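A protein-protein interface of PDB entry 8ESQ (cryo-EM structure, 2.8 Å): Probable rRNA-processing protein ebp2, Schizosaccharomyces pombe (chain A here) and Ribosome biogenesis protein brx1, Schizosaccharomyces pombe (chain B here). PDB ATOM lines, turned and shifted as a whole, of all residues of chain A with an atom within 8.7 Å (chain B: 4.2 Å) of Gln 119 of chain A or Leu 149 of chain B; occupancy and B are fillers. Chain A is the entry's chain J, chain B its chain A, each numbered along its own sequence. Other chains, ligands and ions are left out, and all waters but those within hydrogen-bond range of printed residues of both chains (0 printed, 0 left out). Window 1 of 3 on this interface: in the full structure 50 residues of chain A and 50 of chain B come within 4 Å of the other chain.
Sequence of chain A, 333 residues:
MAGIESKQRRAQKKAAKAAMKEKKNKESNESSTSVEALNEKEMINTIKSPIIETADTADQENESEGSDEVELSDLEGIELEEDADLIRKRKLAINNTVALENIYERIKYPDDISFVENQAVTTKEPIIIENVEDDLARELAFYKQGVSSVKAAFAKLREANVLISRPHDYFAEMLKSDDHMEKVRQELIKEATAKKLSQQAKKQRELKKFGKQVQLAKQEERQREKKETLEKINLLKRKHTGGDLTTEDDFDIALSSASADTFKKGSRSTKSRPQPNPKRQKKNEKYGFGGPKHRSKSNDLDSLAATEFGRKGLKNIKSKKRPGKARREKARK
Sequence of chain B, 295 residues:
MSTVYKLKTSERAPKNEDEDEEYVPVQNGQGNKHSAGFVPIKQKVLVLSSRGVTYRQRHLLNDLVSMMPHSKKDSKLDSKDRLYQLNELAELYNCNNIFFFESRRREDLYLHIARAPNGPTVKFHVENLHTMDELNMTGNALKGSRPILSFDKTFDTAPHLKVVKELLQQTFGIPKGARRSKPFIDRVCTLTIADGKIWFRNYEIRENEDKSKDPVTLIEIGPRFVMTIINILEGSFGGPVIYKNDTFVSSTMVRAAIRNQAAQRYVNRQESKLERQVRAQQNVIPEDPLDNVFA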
ATOM      1  N   TYR A 109       0.646   6.162   5.559  1.00  0.00           N
ATOM      2  CA  TYR A 109      -0.751   5.895   5.849  1.00  0.00           C
ATOM      3  C   TYR A 109      -0.790   5.011   7.087  1.00  0.00           C
ATOM      4  O   TYR A 109      -0.144   3.955   7.096  1.00  0.00           O
ATOM      5  CB  TYR A 109      -1.423   5.210   4.667  1.00  0.00           C
ATOM      6  CG  TYR A 109      -2.766   5.793   4.295  1.00  0.00           C
ATOM      7  CD1 TYR A 109      -2.890   7.132   3.953  1.00  0.00           C
ATOM      8  CD2 TYR A 109      -3.906   5.005   4.274  1.00  0.00           C
ATOM      9  CE1 TYR A 109      -4.113   7.671   3.607  1.00  0.00           C
ATOM     10  CE2 TYR A 109      -5.132   5.532   3.929  1.00  0.00           C
ATOM     11  CZ  TYR A 109      -5.231   6.867   3.596  1.00  0.00           C
ATOM     12  OH  TYR A 109      -6.452   7.397   3.252  1.00  0.00           O
ATOM     13  N   ILE A 113      -5.504   1.993  10.720  1.00  0.00           N
ATOM     14  CA  ILE A 113      -6.758   2.337  10.061  1.00  0.00           C
ATOM     15  C   ILE A 113      -7.511   1.067   9.700  1.00  0.00           C
ATOM     16  O   ILE A 113      -6.917   0.068   9.274  1.00  0.00           O
ATOM     17  CB  ILE A 113      -6.491   3.202   8.821  1.00  0.00           C
ATOM     18  CG1 ILE A 113      -5.589   2.453   7.843  1.00  0.00           C
ATOM     19  CG2 ILE A 113      -5.863   4.528   9.221  1.00  0.00           C
ATOM     20  CD1 ILE A 113      -5.724   2.902   6.426  1.00  0.00           C
ATOM     21  N   SER A 114      -8.826   1.092   9.894  1.00  0.00           N
ATOM     22  CA  SER A 114      -9.653  -0.032   9.487  1.00  0.00           C
ATOM     23  C   SER A 114      -9.606  -0.193   7.973  1.00  0.00           C
ATOM     24  O   SER A 114      -9.368   0.764   7.231  1.00  0.00           O
ATOM     25  CB  SER A 114     -11.094   0.168   9.956  1.00  0.00           C
ATOM     26  OG  SER A 114     -11.807   1.004   9.063  1.00  0.00           O
ATOM     27  N   PHE A 115      -9.823  -1.427   7.515  1.00  0.00           N
ATOM     28  CA  PHE A 115      -9.736  -1.704   6.085  1.00  0.00           C
ATOM     29  C   PHE A 115     -10.766  -0.899   5.305  1.00  0.00           C
ATOM     30  O   PHE A 115     -10.463  -0.372   4.228  1.00  0.00           O
ATOM     31  CB  PHE A 115      -9.899  -3.207   5.831  1.00  0.00           C
ATOM     32  CG  PHE A 115     -10.057  -3.574   4.375  1.00  0.00           C
ATOM     33  CD1 PHE A 115     -11.254  -3.367   3.705  1.00  0.00           C
ATOM     34  CD2 PHE A 115      -9.025  -4.187   3.697  1.00  0.00           C
ATOM     35  CE1 PHE A 115     -11.396  -3.712   2.383  1.00  0.00           C
ATOM     36  CE2 PHE A 115      -9.166  -4.532   2.375  1.00  0.00           C
ATOM     37  CZ  PHE A 115     -10.352  -4.296   1.717  1.00  0.00           C
ATOM     38  N   VAL A 116     -11.992  -0.803   5.825  1.00  0.00           N
ATOM     39  CA  VAL A 116     -13.065  -0.133   5.100  1.00  0.00           C
ATOM     40  C   VAL A 116     -12.734   1.330   4.837  1.00  0.00           C
ATOM     41  O   VAL A 116     -13.232   1.913   3.871  1.00  0.00           O
ATOM     42  CB  VAL A 116     -14.398  -0.284   5.866  1.00  0.00           C
ATOM     43  CG1 VAL A 116     -14.330   0.410   7.217  1.00  0.00           C
ATOM     44  CG2 VAL A 116     -15.564   0.236   5.036  1.00  0.00           C
ATOM     45  N   GLU A 117     -11.880   1.936   5.663  1.00  0.00           N
ATOM     46  CA  GLU A 117     -11.426   3.294   5.384  1.00  0.00           C
ATOM     47  C   GLU A 117     -10.523   3.344   4.157  1.00  0.00           C
ATOM     48  O   GLU A 117     -10.532   4.337   3.422  1.00  0.00           O
ATOM     49  CB  GLU A 117     -10.695   3.866   6.600  1.00  0.00           C
ATOM     50  CG  GLU A 117     -11.546   3.964   7.852  1.00  0.00           C
ATOM     51  CD  GLU A 117     -12.548   5.097   7.781  1.00  0.00           C
ATOM     52  OE1 GLU A 117     -12.265   6.097   7.088  1.00  0.00           O
ATOM     53  OE2 GLU A 117     -13.621   4.989   8.412  1.00  0.00           O
ATOM     54  N   ASN A 118      -9.740   2.292   3.918  1.00  0.00           N
ATOM     55  CA  ASN A 118      -8.699   2.327   2.898  1.00  0.00           C
ATOM     56  C   ASN A 118      -9.031   1.423   1.715  1.00  0.00           C
ATOM     57  O   ASN A 118      -9.029   1.882   0.569  1.00  0.00           O
ATOM     58  CB  ASN A 118      -7.363   1.936   3.557  1.00  0.00           C
ATOM     59  CG  ASN A 118      -6.283   1.452   2.578  1.00  0.00           C
ATOM     60  OD1 ASN A 118      -6.521   1.160   1.413  1.00  0.00           O
ATOM     61  ND2 ASN A 118      -5.065   1.355   3.090  1.00  0.00           N
ATOM     62  N   GLN A 119      -9.274   0.136   1.973  1.00  0.00           N
ATOM     63  CA  GLN A 119      -9.560  -0.862   0.937  1.00  0.00           C
ATOM     64  C   GLN A 119      -8.351  -1.132   0.039  1.00  0.00           C
ATOM     65  O   GLN A 119      -8.487  -1.240  -1.183  1.00  0.00           O
ATOM     66  CB  GLN A 119     -10.773  -0.463   0.089  1.00  0.00           C
ATOM     67  CG  GLN A 119     -12.069  -0.311   0.871  1.00  0.00           C
ATOM     68  CD  GLN A 119     -13.266  -0.044  -0.023  1.00  0.00           C
ATOM     69  OE1 GLN A 119     -13.144  -0.009  -1.246  1.00  0.00           O
ATOM     70  NE2 GLN A 119     -14.427   0.159   0.588  1.00  0.00           N
ATOM     71  N   ALA A 120      -7.158  -1.237   0.623  1.00  0.00           N
ATOM     72  CA  ALA A 120      -5.978  -1.728  -0.080  1.00  0.00           C
ATOM     73  C   ALA A 120      -5.415  -2.922   0.674  1.00  0.00           C
ATOM     74  O   ALA A 120      -5.315  -2.892   1.906  1.00  0.00           O
ATOM     75  CB  ALA A 120      -4.901  -0.650  -0.234  1.00  0.00           C
ATOM     76  N   VAL A 121      -5.066  -3.976  -0.060  1.00  0.00           N
ATOM     77  CA  VAL A 121      -4.500  -5.187   0.520  1.00  0.00           C
ATOM     78  C   VAL A 121      -3.124  -5.408  -0.091  1.00  0.00           C
ATOM     79  O   VAL A 121      -2.898  -5.099  -1.267  1.00  0.00           O
ATOM     80  CB  VAL A 121      -5.398  -6.421   0.302  1.00  0.00           C
ATOM     81  CG1 VAL A 121      -6.853  -6.084   0.546  1.00  0.00           C
ATOM     82  CG2 VAL A 121      -5.201  -7.011  -1.078  1.00  0.00           C
ATOM     83  N   THR A 122      -2.192  -5.875   0.731  1.00  0.00           N
ATOM     84  CA  THR A 122      -0.903  -6.367   0.268  1.00  0.00           C
ATOM     85  C   THR A 122      -0.945  -7.890   0.338  1.00  0.00           C
ATOM     86  O   THR A 122      -0.943  -8.466   1.431  1.00  0.00           O
ATOM     87  CB  THR A 122       0.234  -5.801   1.114  1.00  0.00           C
ATOM     88  OG1 THR A 122       0.199  -4.370   1.065  1.00  0.00           O
ATOM     89  CG2 THR A 122       1.580  -6.293   0.603  1.00  0.00           C
ATOM     90  N   THR A 123      -0.994  -8.537  -0.825  1.00  0.00           N
ATOM     91  CA  THR A 123      -1.122  -9.988  -0.870  1.00  0.00           C
ATOM     92  C   THR A 123       0.064 -10.654  -0.186  1.00  0.00           C
ATOM     93  O   THR A 123       1.221 -10.293  -0.425  1.00  0.00           O
ATOM     94  CB  THR A 123      -1.234 -10.464  -2.319  1.00  0.00           C
ATOM     95  OG1 THR A 123      -0.172  -9.894  -3.094  1.00  0.00           O
ATOM     96  CG2 THR A 123      -2.571 -10.052  -2.915  1.00  0.00           C
ATOM     97  N   GLN A 145      -3.921 -13.804  -7.808  1.00  0.00           N
ATOM     98  CA  GLN A 145      -3.615 -12.766  -6.832  1.00  0.00           C
ATOM     99  C   GLN A 145      -4.849 -11.928  -6.533  1.00  0.00           C
ATOM    100  O   GLN A 145      -5.028 -11.452  -5.405  1.00  0.00           O
ATOM    101  CB  GLN A 145      -2.461 -11.887  -7.320  1.00  0.00           C
ATOM    102  CG  GLN A 145      -2.867 -10.657  -8.115  1.00  0.00           C
ATOM    103  CD  GLN A 145      -2.088  -9.423  -7.705  1.00  0.00           C
ATOM    104  OE1 GLN A 145      -1.646  -9.305  -6.563  1.00  0.00           O
ATOM    105  NE2 GLN A 145      -1.924  -8.491  -8.635  1.00  0.00           N
ATOM    106  N   GLY A 146      -5.711 -11.733  -7.533  1.00  0.00           N
ATOM    107  CA  GLY A 146      -6.932 -10.983  -7.299  1.00  0.00           C
ATOM    108  C   GLY A 146      -7.881 -11.691  -6.354  1.00  0.00           C
ATOM    109  O   GLY A 146      -8.283 -11.128  -5.333  1.00  0.00           O
ATOM    110  N   SER A 149      -6.719 -11.731  -2.926  1.00  0.00           N
ATOM    111  CA  SER A 149      -6.843 -10.384  -2.379  1.00  0.00           C
ATOM    112  C   SER A 149      -8.294 -10.054  -2.054  1.00  0.00           C
ATOM    113  O   SER A 149      -8.590  -9.490  -0.994  1.00  0.00           O
ATOM    114  CB  SER A 149      -6.277  -9.370  -3.370  1.00  0.00           C
ATOM    115  OG  SER A 149      -7.055  -9.329  -4.552  1.00  0.00           O
ATOM    116  N   VAL A 150      -9.211 -10.401  -2.957  1.00  0.00           N
ATOM    117  CA  VAL A 150     -10.632 -10.165  -2.721  1.00  0.00           C
ATOM    118  C   VAL A 150     -11.133 -10.986  -1.539  1.00  0.00           C
ATOM    119  O   VAL A 150     -11.905 -10.492  -0.708  1.00  0.00           O
ATOM    120  CB  VAL A 150     -11.430 -10.453  -4.005  1.00  0.00           C
ATOM    121  CG1 VAL A 150     -12.877 -10.113  -3.812  1.00  0.00           C
ATOM    122  CG2 VAL A 150     -10.886  -9.616  -5.142  1.00  0.00           C
ATOM    123  N   ALA A 153     -10.031  -9.396   1.572  1.00  0.00           N
ATOM    124  CA  ALA A 153     -10.792  -8.161   1.733  1.00  0.00           C
ATOM    125  C   ALA A 153     -12.213  -8.441   2.204  1.00  0.00           C
ATOM    126  O   ALA A 153     -12.723  -7.766   3.106  1.00  0.00           O
ATOM    127  CB  ALA A 153     -10.808  -7.392   0.415  1.00  0.00           C
ATOM    128  N   LYS A 156     -12.296  -9.415   5.896  1.00  0.00           N
ATOM    129  CA  LYS A 156     -12.092  -8.278   6.785  1.00  0.00           C
ATOM    130  C   LYS A 156     -13.278  -7.321   6.766  1.00  0.00           C
ATOM    131  O   LYS A 156     -13.444  -6.525   7.697  1.00  0.00           O
ATOM    132  CB  LYS A 156     -10.805  -7.543   6.411  1.00  0.00           C
ATOM    133  CG  LYS A 156      -9.539  -8.277   6.822  1.00  0.00           C
ATOM    134  CD  LYS A 156      -8.314  -7.384   6.723  1.00  0.00           C
ATOM    135  CE  LYS A 156      -7.836  -7.262   5.287  1.00  0.00           C
ATOM    136  NZ  LYS A 156      -6.481  -6.651   5.205  1.00  0.00           N
ATOM    137  N   LEU A 157     -14.102  -7.374   5.722  1.00  0.00           N
ATOM    138  CA  LEU A 157     -15.246  -6.478   5.614  1.00  0.00           C
ATOM    139  C   LEU A 157     -16.534  -7.072   6.165  1.00  0.00           C
ATOM    140  O   LEU A 157     -17.443  -6.318   6.532  1.00  0.00           O
ATOM    141  CB  LEU A 157     -15.449  -6.059   4.157  1.00  0.00           C
ATOM    142  CG  LEU A 157     -14.533  -4.914   3.731  1.00  0.00           C
ATOM    143  CD1 LEU A 157     -15.114  -4.181   2.551  1.00  0.00           C
ATOM    144  CD2 LEU A 157     -14.344  -3.954   4.895  1.00  0.00           C
ATOM    145  N   VAL A 162     -20.134  -4.124   6.321  1.00  0.00           N
ATOM    146  CA  VAL A 162     -20.349  -3.338   5.114  1.00  0.00           C
ATOM    147  C   VAL A 162     -20.960  -4.239   4.052  1.00  0.00           C
ATOM    148  O   VAL A 162     -20.487  -5.355   3.809  1.00  0.00           O
ATOM    149  CB  VAL A 162     -19.032  -2.705   4.619  1.00  0.00           C
ATOM    150  CG1 VAL A 162     -19.278  -1.870   3.374  1.00  0.00           C
ATOM    151  CG2 VAL A 162     -18.402  -1.873   5.722  1.00  0.00           C
ATOM    152  N   LEU A 163     -22.015  -3.750   3.405  1.00  0.00           N
ATOM    153  CA  LEU A 163     -22.730  -4.542   2.406  1.00  0.00           C
ATOM    154  C   LEU A 163     -21.825  -4.724   1.198  1.00  0.00           C
ATOM    155  O   LEU A 163     -21.647  -3.811   0.391  1.00  0.00           O
ATOM    156  CB  LEU A 163     -24.050  -3.890   2.013  1.00  0.00           C
ATOM    157  CG  LEU A 163     -25.131  -3.605   3.062  1.00  0.00           C
ATOM    158  CD1 LEU A 163     -24.790  -2.433   3.982  1.00  0.00           C
ATOM    159  CD2 LEU A 163     -26.476  -3.402   2.380  1.00  0.00           C
ATOM    160  N   ILE A 164     -21.240  -5.915   1.080  1.00  0.00           N
ATOM    161  CA  ILE A 164     -20.358  -6.198  -0.045  1.00  0.00           C
ATOM    162  C   ILE A 164     -21.148  -6.248  -1.345  1.00  0.00           C
ATOM    163  O   ILE A 164     -20.758  -5.645  -2.352  1.00  0.00           O
ATOM    164  CB  ILE A 164     -19.592  -7.510   0.197  1.00  0.00           C
ATOM    165  CG1 ILE A 164     -18.603  -7.364   1.361  1.00  0.00           C
ATOM    166  CG2 ILE A 164     -18.908  -7.951  -1.071  1.00  0.00           C
ATOM    167  CD1 ILE A 164     -18.087  -5.955   1.581  1.00  0.00           C
ATOM    168  N   ARG B 146     -16.206   2.590  -4.033  1.00  0.00           N
ATOM    169  CA  ARG B 146     -14.869   2.457  -3.483  1.00  0.00           C
ATOM    170  C   ARG B 146     -14.300   1.092  -3.851  1.00  0.00           C
ATOM    171  O   ARG B 146     -14.892   0.064  -3.491  1.00  0.00           O
ATOM    172  CB  ARG B 146     -14.909   2.640  -1.970  1.00  0.00           C
ATOM    173  CG  ARG B 146     -15.538   3.957  -1.553  1.00  0.00           C
ATOM    174  CD  ARG B 146     -15.537   4.134  -0.051  1.00  0.00           C
ATOM    175  NE  ARG B 146     -14.194   4.389   0.454  1.00  0.00           N
ATOM    176  CZ  ARG B 146     -13.674   3.804   1.523  1.00  0.00           C
ATOM    177  NH1 ARG B 146     -14.362   2.922   2.229  1.00  0.00           N
ATOM    178  NH2 ARG B 146     -12.436   4.113   1.893  1.00  0.00           N
ATOM    179  N   PRO B 147     -13.180   1.031  -4.562  1.00  0.00           N
ATOM    180  CA  PRO B 147     -12.643  -0.252  -5.009  1.00  0.00           C
ATOM    181  C   PRO B 147     -11.629  -0.816  -4.021  1.00  0.00           C
ATOM    182  O   PRO B 147     -11.058  -0.104  -3.192  1.00  0.00           O
ATOM    183  CB  PRO B 147     -11.966   0.118  -6.332  1.00  0.00           C
ATOM    184  CG  PRO B 147     -11.445   1.496  -6.076  1.00  0.00           C
ATOM    185  CD  PRO B 147     -12.406   2.161  -5.105  1.00  0.00           C
ATOM    186  N   ILE B 148     -11.410  -2.119  -4.133  1.00  0.00           N
ATOM    187  CA  ILE B 148     -10.394  -2.803  -3.346  1.00  0.00           C
ATOM    188  C   ILE B 148      -9.078  -2.736  -4.104  1.00  0.00           C
ATOM    189  O   ILE B 148      -9.006  -3.117  -5.278  1.00  0.00           O
ATOM    190  CB  ILE B 148     -10.797  -4.259  -3.067  1.00  0.00           C
ATOM    191  CG1 ILE B 148     -12.256  -4.333  -2.613  1.00  0.00           C
ATOM    192  CG2 ILE B 148      -9.876  -4.869  -2.025  1.00  0.00           C
ATOM    193  CD1 ILE B 148     -12.830  -5.731  -2.632  1.00  0.00           C
ATOM    194  N   LEU B 149      -8.038  -2.247  -3.440  1.00  0.00           N
ATOM    195  CA  LEU B 149      -6.722  -2.104  -4.048  1.00  0.00           C
ATOM    196  C   LEU B 149      -5.873  -3.308  -3.663  1.00  0.00           C
ATOM    197  O   LEU B 149      -5.806  -3.675  -2.486  1.00  0.00           O
ATOM    198  CB  LEU B 149      -6.052  -0.806  -3.601  1.00  0.00           C
ATOM    199  CG  LEU B 149      -6.627   0.506  -4.134  1.00  0.00           C
ATOM    200  CD1 LEU B 149      -5.695   1.668  -3.818  1.00  0.00           C
ATOM    201  CD2 LEU B 149      -6.889   0.414  -5.625  1.00  0.00           C
ATOM    202  N   SER B 150      -5.248  -3.934  -4.653  1.00  0.00           N
ATOM    203  CA  SER B 150      -4.322  -5.033  -4.422  1.00  0.00           C
ATOM    204  C   SER B 150      -2.941  -4.629  -4.913  1.00  0.00           C
ATOM    205  O   SER B 150      -2.774  -4.267  -6.082  1.00  0.00           O
ATOM    206  CB  SER B 150      -4.793  -6.308  -5.126  1.00  0.00           C
ATOM    207  OG  SER B 150      -4.942  -6.097  -6.515  1.00  0.00           O
ATOM    208  N   PHE B 151      -1.957  -4.694  -4.021  1.00  0.00           N
ATOM    209  CA  PHE B 151      -0.590  -4.298  -4.323  1.00  0.00           C
ATOM    210  C   PHE B 151       0.306  -5.527  -4.325  1.00  0.00           C
ATOM    211  O   PHE B 151       0.231  -6.356  -3.412  1.00  0.00           O
ATOM    212  CB  PHE B 151      -0.074  -3.276  -3.308  1.00  0.00           C
ATOM    213  CG  PHE B 151      -0.686  -1.915  -3.454  1.00  0.00           C
ATOM    214  CD1 PHE B 151      -0.311  -1.083  -4.494  1.00  0.00           C
ATOM    215  CD2 PHE B 151      -1.630  -1.465  -2.547  1.00  0.00           C
ATOM    216  CE1 PHE B 151      -0.870   0.171  -4.631  1.00  0.00           C
ATOM    217  CE2 PHE B 151      -2.191  -0.212  -2.679  1.00  0.00           C
ATOM    218  CZ  PHE B 151      -1.811   0.607  -3.724  1.00  0.00           C
ATOM    219  N   GLN B 169      -1.807   4.233  -3.476  1.00  0.00           N
ATOM    220  CA  GLN B 169      -2.890   3.862  -2.572  1.00  0.00           C
ATOM    221  C   GLN B 169      -3.685   5.088  -2.139  1.00  0.00           C
ATOM    222  O   GLN B 169      -4.921   5.070  -2.128  1.00  0.00           O
ATOM    223  CB  GLN B 169      -2.326   3.130  -1.355  1.00  0.00           C
ATOM    224  CG  GLN B 169      -3.290   3.022  -0.188  1.00  0.00           C
ATOM    225  CD  GLN B 169      -2.609   2.565   1.084  1.00  0.00           C
ATOM    226  OE1 GLN B 169      -3.032   2.909   2.186  1.00  0.00           O
ATOM    227  NE2 GLN B 169      -1.545   1.785   0.937  1.00  0.00           N
ATOM    228  N   PHE B 172      -5.883   6.187  -5.545  1.00  0.00           N
ATOM    229  CA  PHE B 172      -6.941   5.327  -6.071  1.00  0.00           C
ATOM    230  C   PHE B 172      -7.966   4.972  -5.004  1.00  0.00           C
ATOM    231  O   PHE B 172      -9.167   4.903  -5.291  1.00  0.00           O
ATOM    232  CB  PHE B 172      -6.342   4.063  -6.681  1.00  0.00           C
ATOM    233  CG  PHE B 172      -5.761   4.271  -8.046  1.00  0.00           C
ATOM    234  CD1 PHE B 172      -6.566   4.676  -9.096  1.00  0.00           C
ATOM    235  CD2 PHE B 172      -4.415   4.061  -8.282  1.00  0.00           C
ATOM    236  CE1 PHE B 172      -6.040   4.870 -10.355  1.00  0.00           C
ATOM    237  CE2 PHE B 172      -3.885   4.252  -9.542  1.00  0.00           C
ATOM    238  CZ  PHE B 172      -4.697   4.658 -10.578  1.00  0.00           C
ATOM    239  N   GLY B 173      -7.519   4.723  -3.777  1.00  0.00           N
ATOM    240  CA  GLY B 173      -8.442   4.447  -2.697  1.00  0.00           C
ATOM    241  C   GLY B 173      -9.389   5.604  -2.466  1.00  0.00           C
ATOM    242  O   GLY B 173      -8.980   6.654  -1.961  1.00  0.00           O
ATOM    243  N   ILE B 185     -19.360  -2.055  -3.052  1.00  0.00           N
ATOM    244  CA  ILE B 185     -18.062  -2.352  -3.644  1.00  0.00           C
ATOM    245  C   ILE B 185     -18.271  -3.299  -4.815  1.00  0.00           C
ATOM    246  O   ILE B 185     -18.910  -4.347  -4.668  1.00  0.00           O
ATOM    247  CB  ILE B 185     -17.104  -2.965  -2.610  1.00  0.00           C
ATOM    248  CG1 ILE B 185     -16.707  -1.915  -1.578  1.00  0.00           C
ATOM    249  CG2 ILE B 185     -15.875  -3.547  -3.294  1.00  0.00           C
ATOM    250  CD1 ILE B 185     -15.990  -2.487  -0.401  1.00  0.00           C
ATOM    251  N   CYS B 189      -8.762  -3.071  -8.150  1.00  0.00           N
ATOM    252  CA  CYS B 189      -7.662  -2.577  -8.967  1.00  0.00           C
ATOM    253  C   CYS B 189      -6.387  -3.305  -8.565  1.00  0.00           C
ATOM    254  O   CYS B 189      -6.022  -3.318  -7.384  1.00  0.00           O
ATOM    255  CB  CYS B 189      -7.499  -1.068  -8.795  1.00  0.00           C
ATOM    256  SG  CYS B 189      -8.243  -0.089 -10.112  1.00  0.00           S
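Of the 22 printed residues of chain A, 14 touch a printed residue of chain B.
Of the 11 printed residues of chain B, 8 touch a printed residue of chain A.
Printed residues of chain B that touch a printed residue of chain A: Arg 146, Pro 147, Ile 148, Leu 149, Ser 150, Phe 151, Gln 169 and Ile 185.
Among the printed residues, 22 pairs touch across the chains.
Among the printed residues, no Asp or Glu carboxylate lies within 4 Å of a Lys or Arg side-chain nitrogen of the other chain.
Printed residues of chain B within 4 Å of Tyr 109 of chain A: Gln 169.
Gln 119 of chain A touches just these residues of chain B: Arg 146 (2.8 Å), Pro 147 (2.9 Å), Ile 148 (3.3 Å), Leu 149 (2.5 Å) and Ile 185 (3.2 Å).
Printed residues of chain B within 4 Å of Ile 164 of chain A: Ile 185.
Printed residues of chain A within 4 Å of Ile 148 of chain B: Phe 115 (3.8 Å), Gln 119 (3.3 Å) and Ala 153 (3.6 Å).
Of chain A, only Gln 119, Ala 120 and Val 121 come within 4 Å of Leu 149 of chain B.
Of the printed residues of chain A, Ile 185 of chain B touches Gln 119 (3.2 Å), Leu 157 (3.5 Å) and Ile 164 (3.2 Å).
The nearest printed residue of chain B that does not touch Leu 157 of chain A is Ile 148 of chain B (5.9 Å).
CG2 of Ile 148 of chain B touches CZ of Phe 115 of chain A, 3.8 Å away.
Asn 118 of chain A touches Arg 146 of chain B (N to NH2, 3.8 Å).
Gln 119 of chain A touches Ile 185 of chain B (NE2 to CD1, 3.2 Å).
Ala 120 of chain A touches Leu 149 of chain B (CA to O, 3.1 Å).
Ala 120 of chain A touches Phe 151 of chain B.
Phe 151 of chain B touches Thr 122 of chain A.
Phe 151 of chain B touches Thr 123 of chain A.
Ser 150 of chain B touches Ser 149 of chain A (CB to OG, 3.8 Å).
CB of Ala 153 of chain A touches CG2 of Ile 148 of chain B, at 3.6 Å.
CD1 of Leu 157 of chain A touches CD1 of Ile 185 of chain B, at 3.5 Å.
The guanidinium group (NH2) of Arg 146 of chain B lies close to the backbone carbonyl oxygen (O) of Val 116 of chain A, 3.1 Å away.
The guanidinium group of Arg 146 of chain B is in hydrogen-bond range of the backbone carbonyl oxygen of Glu 117 of chain A, at 2.5 Å.
The side-chain amide oxygen (OE1) of Gln 169 of chain B lies within hydrogen-bond range of the side-chain amide nitrogen (ND2) of Asn 118 of chain A.
The side-chain amide oxygen of Gln 119 of chain A lies close to the backbone carbonyl oxygen of Arg 146 of chain B, 2.8 Å away.
OE1 of Gln 119 of chain A sits close to O of Pro 147 of chain B (2.9 Å).
The backbone carbonyl oxygen (O) of Gln 119 of chain A lies within hydrogen-bond range of the backbone NH (N) of Leu 149 of chain B, at 2.5 Å.
The backbone NH (N) of Val 121 of chain A sits at hydrogen-bond distance from the backbone carbonyl oxygen (O) of Leu 149 of chain B (2.6 Å).
The backbone carbonyl oxygen of Val 121 of chain A is in hydrogen-bond range of the backbone NH of Phe 151 of chain B, at 2.9 Å.
The backbone carbonyl oxygen (O) of Ile 164 of chain A lies close to the backbone carbonyl oxygen (O) of Ile 185 of chain B (3.2 Å).
N of Ala 120 of chain A lies within hydrogen-bond range of OD1 of Asn 118 of chain A.
The side-chain hydroxyl (OG) of Ser 149 of chain A lies within hydrogen-bond range of the backbone carbonyl oxygen (O) of Gln 145 of chain A.
The backbone carbonyl oxygen (O) of Leu 157 of chain A lies within hydrogen-bond range of the backbone NH (N) of Val 162 of chain A.
The backbone carbonyl oxygen (O) of Ile 148 of chain B is in hydrogen-bond range of the backbone NH (N) of Cys 189 of chain B (2.9 Å).
N of Ser 150 of chain B lies within hydrogen-bond range of O of Cys 189 of chain B, at 2.9 Å.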
